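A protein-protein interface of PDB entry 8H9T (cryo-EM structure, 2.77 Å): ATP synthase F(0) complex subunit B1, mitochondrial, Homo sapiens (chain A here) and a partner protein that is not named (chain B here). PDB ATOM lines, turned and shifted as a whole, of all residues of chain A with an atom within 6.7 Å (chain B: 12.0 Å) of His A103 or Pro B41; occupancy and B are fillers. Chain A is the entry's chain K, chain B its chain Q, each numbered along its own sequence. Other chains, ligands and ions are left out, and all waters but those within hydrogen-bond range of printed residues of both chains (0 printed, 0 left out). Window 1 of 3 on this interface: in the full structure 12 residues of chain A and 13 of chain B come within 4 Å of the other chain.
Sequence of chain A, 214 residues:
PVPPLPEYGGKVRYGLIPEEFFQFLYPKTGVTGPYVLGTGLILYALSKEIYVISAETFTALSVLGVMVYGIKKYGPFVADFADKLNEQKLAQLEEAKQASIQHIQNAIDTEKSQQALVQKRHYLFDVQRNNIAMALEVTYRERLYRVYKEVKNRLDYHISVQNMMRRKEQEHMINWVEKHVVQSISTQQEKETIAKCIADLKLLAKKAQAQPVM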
ATOM      1  N   GLN A  98     -22.132   8.609  27.494  1.00  0.00           N
ATOM      2  CA  GLN A  98     -20.730   9.009  27.430  1.00  0.00           C
ATOM      3  C   GLN A  98     -20.208   8.980  26.004  1.00  0.00           C
ATOM      4  O   GLN A  98     -19.457   9.871  25.592  1.00  0.00           O
ATOM      5  CB  GLN A  98     -19.886   8.100  28.314  1.00  0.00           C
ATOM      6  CG  GLN A  98     -20.169   8.254  29.780  1.00  0.00           C
ATOM      7  CD  GLN A  98     -20.107   9.692  30.220  1.00  0.00           C
ATOM      8  OE1 GLN A  98     -21.000  10.182  30.907  1.00  0.00           O
ATOM      9  NE2 GLN A  98     -19.047  10.384  29.827  1.00  0.00           N
ATOM     10  N   ALA A  99     -20.582   7.958  25.240  1.00  0.00           N
ATOM     11  CA  ALA A  99     -20.058   7.830  23.888  1.00  0.00           C
ATOM     12  C   ALA A  99     -20.489   9.001  23.021  1.00  0.00           C
ATOM     13  O   ALA A  99     -19.700   9.508  22.218  1.00  0.00           O
ATOM     14  CB  ALA A  99     -20.507   6.512  23.267  1.00  0.00           C
ATOM     15  N   SER A 100     -21.727   9.464  23.179  1.00  0.00           N
ATOM     16  CA  SER A 100     -22.174  10.567  22.337  1.00  0.00           C
ATOM     17  C   SER A 100     -21.562  11.886  22.794  1.00  0.00           C
ATOM     18  O   SER A 100     -21.272  12.764  21.966  1.00  0.00           O
ATOM     19  CB  SER A 100     -23.696  10.644  22.325  1.00  0.00           C
ATOM     20  OG  SER A 100     -24.130  11.680  21.464  1.00  0.00           O
ATOM     21  N   ILE A 101     -21.343  12.045  24.102  1.00  0.00           N
ATOM     22  CA  ILE A 101     -20.582  13.205  24.566  1.00  0.00           C
ATOM     23  C   ILE A 101     -19.214  13.230  23.898  1.00  0.00           C
ATOM     24  O   ILE A 101     -18.774  14.259  23.367  1.00  0.00           O
ATOM     25  CB  ILE A 101     -20.457  13.195  26.098  1.00  0.00           C
ATOM     26  CG1 ILE A 101     -21.681  13.831  26.736  1.00  0.00           C
ATOM     27  CG2 ILE A 101     -19.222  13.947  26.534  1.00  0.00           C
ATOM     28  CD1 ILE A 101     -21.735  13.635  28.223  1.00  0.00           C
ATOM     29  N   GLN A 102     -18.523  12.090  23.918  1.00  0.00           N
ATOM     30  CA  GLN A 102     -17.214  12.008  23.285  1.00  0.00           C
ATOM     31  C   GLN A 102     -17.306  12.313  21.803  1.00  0.00           C
ATOM     32  O   GLN A 102     -16.418  12.958  21.240  1.00  0.00           O
ATOM     33  CB  GLN A 102     -16.607  10.625  23.498  1.00  0.00           C
ATOM     34  CG  GLN A 102     -15.972  10.446  24.854  1.00  0.00           C
ATOM     35  CD  GLN A 102     -15.181  11.659  25.276  1.00  0.00           C
ATOM     36  OE1 GLN A 102     -14.127  11.950  24.715  1.00  0.00           O
ATOM     37  NE2 GLN A 102     -15.688  12.381  26.266  1.00  0.00           N
ATOM     38  N   HIS A 103     -18.368  11.849  21.152  1.00  0.00           N
ATOM     39  CA  HIS A 103     -18.542  12.148  19.740  1.00  0.00           C
ATOM     40  C   HIS A 103     -18.573  13.646  19.499  1.00  0.00           C
ATOM     41  O   HIS A 103     -17.862  14.165  18.629  1.00  0.00           O
ATOM     42  CB  HIS A 103     -19.829  11.542  19.215  1.00  0.00           C
ATOM     43  CG  HIS A 103     -20.262  12.133  17.914  1.00  0.00           C
ATOM     44  ND1 HIS A 103     -19.739  11.729  16.707  1.00  0.00           N
ATOM     45  CD2 HIS A 103     -21.139  13.126  17.632  1.00  0.00           C
ATOM     46  CE1 HIS A 103     -20.292  12.432  15.736  1.00  0.00           C
ATOM     47  NE2 HIS A 103     -21.144  13.286  16.270  1.00  0.00           N
ATOM     48  N   ILE A 104     -19.428  14.354  20.232  1.00  0.00           N
ATOM     49  CA  ILE A 104     -19.570  15.784  19.977  1.00  0.00           C
ATOM     50  C   ILE A 104     -18.273  16.514  20.296  1.00  0.00           C
ATOM     51  O   ILE A 104     -17.872  17.443  19.580  1.00  0.00           O
ATOM     52  CB  ILE A 104     -20.760  16.357  20.761  1.00  0.00           C
ATOM     53  CG1 ILE A 104     -22.057  15.730  20.262  1.00  0.00           C
ATOM     54  CG2 ILE A 104     -20.834  17.855  20.578  1.00  0.00           C
ATOM     55  CD1 ILE A 104     -22.360  16.063  18.825  1.00  0.00           C
ATOM     56  N   GLN A 105     -17.576  16.094  21.349  1.00  0.00           N
ATOM     57  CA  GLN A 105     -16.317  16.756  21.665  1.00  0.00           C
ATOM     58  C   GLN A 105     -15.279  16.516  20.577  1.00  0.00           C
ATOM     59  O   GLN A 105     -14.525  17.428  20.217  1.00  0.00           O
ATOM     60  CB  GLN A 105     -15.795  16.292  23.019  1.00  0.00           C
ATOM     61  CG  GLN A 105     -14.565  17.048  23.485  1.00  0.00           C
ATOM     62  CD  GLN A 105     -14.886  18.432  24.015  1.00  0.00           C
ATOM     63  OE1 GLN A 105     -15.845  19.071  23.590  1.00  0.00           O
ATOM     64  NE2 GLN A 105     -14.073  18.903  24.949  1.00  0.00           N
ATOM     65  N   ASN A 106     -15.223  15.297  20.043  1.00  0.00           N
ATOM     66  CA  ASN A 106     -14.283  15.019  18.967  1.00  0.00           C
ATOM     67  C   ASN A 106     -14.607  15.848  17.737  1.00  0.00           C
ATOM     68  O   ASN A 106     -13.699  16.350  17.063  1.00  0.00           O
ATOM     69  CB  ASN A 106     -14.296  13.533  18.631  1.00  0.00           C
ATOM     70  CG  ASN A 106     -13.710  12.693  19.735  1.00  0.00           C
ATOM     71  OD1 ASN A 106     -13.297  13.215  20.767  1.00  0.00           O
ATOM     72  ND2 ASN A 106     -13.666  11.382  19.528  1.00  0.00           N
ATOM     73  N   ALA A 107     -15.893  16.013  17.431  1.00  0.00           N
ATOM     74  CA  ALA A 107     -16.260  16.852  16.293  1.00  0.00           C
ATOM     75  C   ALA A 107     -15.819  18.292  16.514  1.00  0.00           C
ATOM     76  O   ALA A 107     -15.290  18.935  15.597  1.00  0.00           O
ATOM     77  CB  ALA A 107     -17.763  16.784  16.045  1.00  0.00           C
ATOM     78  N   ILE A 108     -16.009  18.810  17.729  1.00  0.00           N
ATOM     79  CA  ILE A 108     -15.594  20.181  18.024  1.00  0.00           C
ATOM     80  C   ILE A 108     -14.090  20.336  17.836  1.00  0.00           C
ATOM     81  O   ILE A 108     -13.617  21.281  17.191  1.00  0.00           O
ATOM     82  CB  ILE A 108     -16.014  20.576  19.447  1.00  0.00           C
ATOM     83  CG1 ILE A 108     -17.510  20.852  19.507  1.00  0.00           C
ATOM     84  CG2 ILE A 108     -15.251  21.792  19.904  1.00  0.00           C
ATOM     85  CD1 ILE A 108     -17.973  21.268  20.875  1.00  0.00           C
ATOM     86  N   PRO B  36     -31.911  -0.500  21.117  1.00  0.00           N
ATOM     87  CA  PRO B  36     -30.832  -0.150  22.033  1.00  0.00           C
ATOM     88  C   PRO B  36     -30.171   1.148  21.615  1.00  0.00           C
ATOM     89  O   PRO B  36     -30.121   1.470  20.420  1.00  0.00           O
ATOM     90  CB  PRO B  36     -29.859  -1.330  21.908  1.00  0.00           C
ATOM     91  CG  PRO B  36     -30.643  -2.417  21.281  1.00  0.00           C
ATOM     92  CD  PRO B  36     -31.632  -1.747  20.394  1.00  0.00           C
ATOM     93  N   PRO B  37     -29.656   1.923  22.568  1.00  0.00           N
ATOM     94  CA  PRO B  37     -28.958   3.163  22.212  1.00  0.00           C
ATOM     95  C   PRO B  37     -27.654   2.826  21.510  1.00  0.00           C
ATOM     96  O   PRO B  37     -26.785   2.159  22.073  1.00  0.00           O
ATOM     97  CB  PRO B  37     -28.728   3.839  23.564  1.00  0.00           C
ATOM     98  CG  PRO B  37     -28.694   2.731  24.528  1.00  0.00           C
ATOM     99  CD  PRO B  37     -29.571   1.635  24.005  1.00  0.00           C
ATOM    100  N   SER B  38     -27.519   3.262  20.256  1.00  0.00           N
ATOM    101  CA  SER B  38     -26.254   3.038  19.507  1.00  0.00           C
ATOM    102  C   SER B  38     -25.515   4.371  19.335  1.00  0.00           C
ATOM    103  O   SER B  38     -25.496   4.893  18.203  1.00  0.00           O
ATOM    104  CB  SER B  38     -26.525   2.386  18.177  1.00  0.00           C
ATOM    105  OG  SER B  38     -25.320   2.213  17.445  1.00  0.00           O
ATOM    106  N   PRO B  39     -24.908   4.944  20.400  1.00  0.00           N
ATOM    107  CA  PRO B  39     -24.242   6.244  20.305  1.00  0.00           C
ATOM    108  C   PRO B  39     -22.990   6.135  19.426  1.00  0.00           C
ATOM    109  O   PRO B  39     -21.942   5.836  19.962  1.00  0.00           O
ATOM    110  CB  PRO B  39     -23.847   6.557  21.754  1.00  0.00           C
ATOM    111  CG  PRO B  39     -23.719   5.194  22.396  1.00  0.00           C
ATOM    112  CD  PRO B  39     -24.801   4.363  21.740  1.00  0.00           C
ATOM    113  N   LYS B  40     -23.132   6.370  18.119  1.00  0.00           N
ATOM    114  CA  LYS B  40     -22.009   6.265  17.197  1.00  0.00           C
ATOM    115  C   LYS B  40     -21.084   7.442  17.435  1.00  0.00           C
ATOM    116  O   LYS B  40     -21.386   8.563  16.983  1.00  0.00           O
ATOM    117  CB  LYS B  40     -22.506   6.251  15.755  1.00  0.00           C
ATOM    118  CG  LYS B  40     -21.423   6.077  14.716  1.00  0.00           C
ATOM    119  CD  LYS B  40     -22.025   5.657  13.389  1.00  0.00           C
ATOM    120  CE  LYS B  40     -22.777   6.805  12.748  1.00  0.00           C
ATOM    121  NZ  LYS B  40     -21.838   7.806  12.184  1.00  0.00           N
ATOM    122  N   PRO B  41     -19.959   7.260  18.130  1.00  0.00           N
ATOM    123  CA  PRO B  41     -19.028   8.373  18.332  1.00  0.00           C
ATOM    124  C   PRO B  41     -18.349   8.840  17.058  1.00  0.00           C
ATOM    125  O   PRO B  41     -17.545   9.776  17.112  1.00  0.00           O
ATOM    126  CB  PRO B  41     -18.005   7.797  19.323  1.00  0.00           C
ATOM    127  CG  PRO B  41     -18.034   6.335  19.085  1.00  0.00           C
ATOM    128  CD  PRO B  41     -19.441   5.992  18.675  1.00  0.00           C
ATOM    129  N   MET B  42     -18.659   8.227  15.920  1.00  0.00           N
ATOM    130  CA  MET B  42     -18.047   8.558  14.641  1.00  0.00           C
ATOM    131  C   MET B  42     -19.151   8.980  13.675  1.00  0.00           C
ATOM    132  O   MET B  42     -19.679   8.166  12.916  1.00  0.00           O
ATOM    133  CB  MET B  42     -17.259   7.379  14.095  1.00  0.00           C
ATOM    134  CG  MET B  42     -15.929   7.762  13.473  1.00  0.00           C
ATOM    135  SD  MET B  42     -14.837   8.572  14.653  1.00  0.00           S
ATOM    136  CE  MET B  42     -14.722   7.311  15.917  1.00  0.00           C
ATOM    137  N   LYS B  43     -19.506  10.261  13.721  1.00  0.00           N
ATOM    138  CA  LYS B  43     -20.322  10.869  12.670  1.00  0.00           C
ATOM    139  C   LYS B  43     -19.755  12.269  12.428  1.00  0.00           C
ATOM    140  O   LYS B  43     -20.218  13.249  13.013  1.00  0.00           O
ATOM    141  CB  LYS B  43     -21.792  10.910  13.051  1.00  0.00           C
ATOM    142  CG  LYS B  43     -22.681  11.555  12.005  1.00  0.00           C
ATOM    143  CD  LYS B  43     -22.762  10.712  10.750  1.00  0.00           C
ATOM    144  CE  LYS B  43     -23.661  11.374   9.727  1.00  0.00           C
ATOM    145  NZ  LYS B  43     -23.345  12.824   9.593  1.00  0.00           N
ATOM    146  N   MET B  44     -18.765  12.352  11.546  1.00  0.00           N
ATOM    147  CA  MET B  44     -18.134  13.626  11.214  1.00  0.00           C
ATOM    148  C   MET B  44     -17.659  13.565   9.771  1.00  0.00           C
ATOM    149  O   MET B  44     -16.583  13.038   9.479  1.00  0.00           O
ATOM    150  CB  MET B  44     -16.985  13.946  12.161  1.00  0.00           C
ATOM    151  CG  MET B  44     -16.646  15.434  12.238  1.00  0.00           C
ATOM    152  SD  MET B  44     -15.849  16.104  10.760  1.00  0.00           S
ATOM    153  CE  MET B  44     -14.405  15.054  10.635  1.00  0.00           C
ATOM    154  N   LYS B  45     -18.464  14.101   8.867  1.00  0.00           N
ATOM    155  CA  LYS B  45     -17.983  14.460   7.542  1.00  0.00           C
ATOM    156  C   LYS B  45     -18.384  15.913   7.333  1.00  0.00           C
ATOM    157  O   LYS B  45     -19.520  16.223   6.973  1.00  0.00           O
ATOM    158  CB  LYS B  45     -18.536  13.546   6.459  1.00  0.00           C
ATOM    159  CG  LYS B  45     -17.905  13.824   5.111  1.00  0.00           C
ATOM    160  CD  LYS B  45     -16.392  13.747   5.236  1.00  0.00           C
ATOM    161  CE  LYS B  45     -15.693  14.131   3.949  1.00  0.00           C
ATOM    162  NZ  LYS B  45     -14.231  14.288   4.176  1.00  0.00           N
ATOM    163  N   ASN B  46     -17.436  16.811   7.583  1.00  0.00           N
ATOM    164  CA  ASN B  46     -17.659  18.235   7.384  1.00  0.00           C
ATOM    165  C   ASN B  46     -17.206  18.618   5.980  1.00  0.00           C
ATOM    166  O   ASN B  46     -18.044  18.860   5.109  1.00  0.00           O
ATOM    167  CB  ASN B  46     -16.883  18.987   8.476  1.00  0.00           C
ATOM    168  CG  ASN B  46     -16.660  20.461   8.172  1.00  0.00           C
ATOM    169  OD1 ASN B  46     -17.238  21.032   7.249  1.00  0.00           O
ATOM    170  ND2 ASN B  46     -15.799  21.086   8.969  1.00  0.00           N
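Hydrophobic or aromatic side chains of chain B within 4 Å of the printed part of chain A: Pro B39 and Pro B41.
Of the 11 printed residues of chain A, 3 touch a printed residue of chain B.
Printed residues of chain A that touch a printed residue of chain B: Ala A99, Ser A100 and His A103.
Hydrophobic or aromatic side chains of chain A within 4 Å of the printed part of chain B: Ala A99 and His A103.
Among the printed residues, 7 pairs touch across the chains.
Among the printed residues, no Asp or Glu carboxylate lies within 4 Å of a Lys or Arg side-chain nitrogen of the other chain.
CB of Ala A99 touches CG of Pro B39, 3.6 Å away.
Ala A99 touches Pro B41 (O to CB, 3.8 Å).
Ser A100 touches Pro B39.
His A103 touches Lys B40.
His A103 touches Met B42 (ND1 to N, 3.7 Å).
The backbone NH of Lys B43 sits close to a ring nitrogen (ND1) of His A103, at 3.3 Å.
A ring nitrogen (ND1) of His A103 is in hydrogen-bond range of the backbone carbonyl oxygen (O) of Pro B41.
No residue of chain B comes within 4 Å of Gln A102.
His A103 touches four residues of chain B.
No residue of chain B comes within 4 Å of Ile A104.
No residue of chain B comes within 4 Å of Asn A106.
Of the printed residues of chain A, Lys B40 touches His A103.
Pro B41 touches just these residues of chain A: Ala A99 and His A103.
Of the printed residues of chain A, Met B42 touches His A103 (3.7 Å).
Printed residues of chain A within 4 Å of Lys B43: His A103 (2.8 Å).
Lys B45 touches none of the printed residues of chain A.
The nearest residue of chain B that does not touch His A103 is Met B44 (4.5 Å).
The nearest residue of chain A that does not touch Pro B41 is Asn A106 (4.8 Å).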
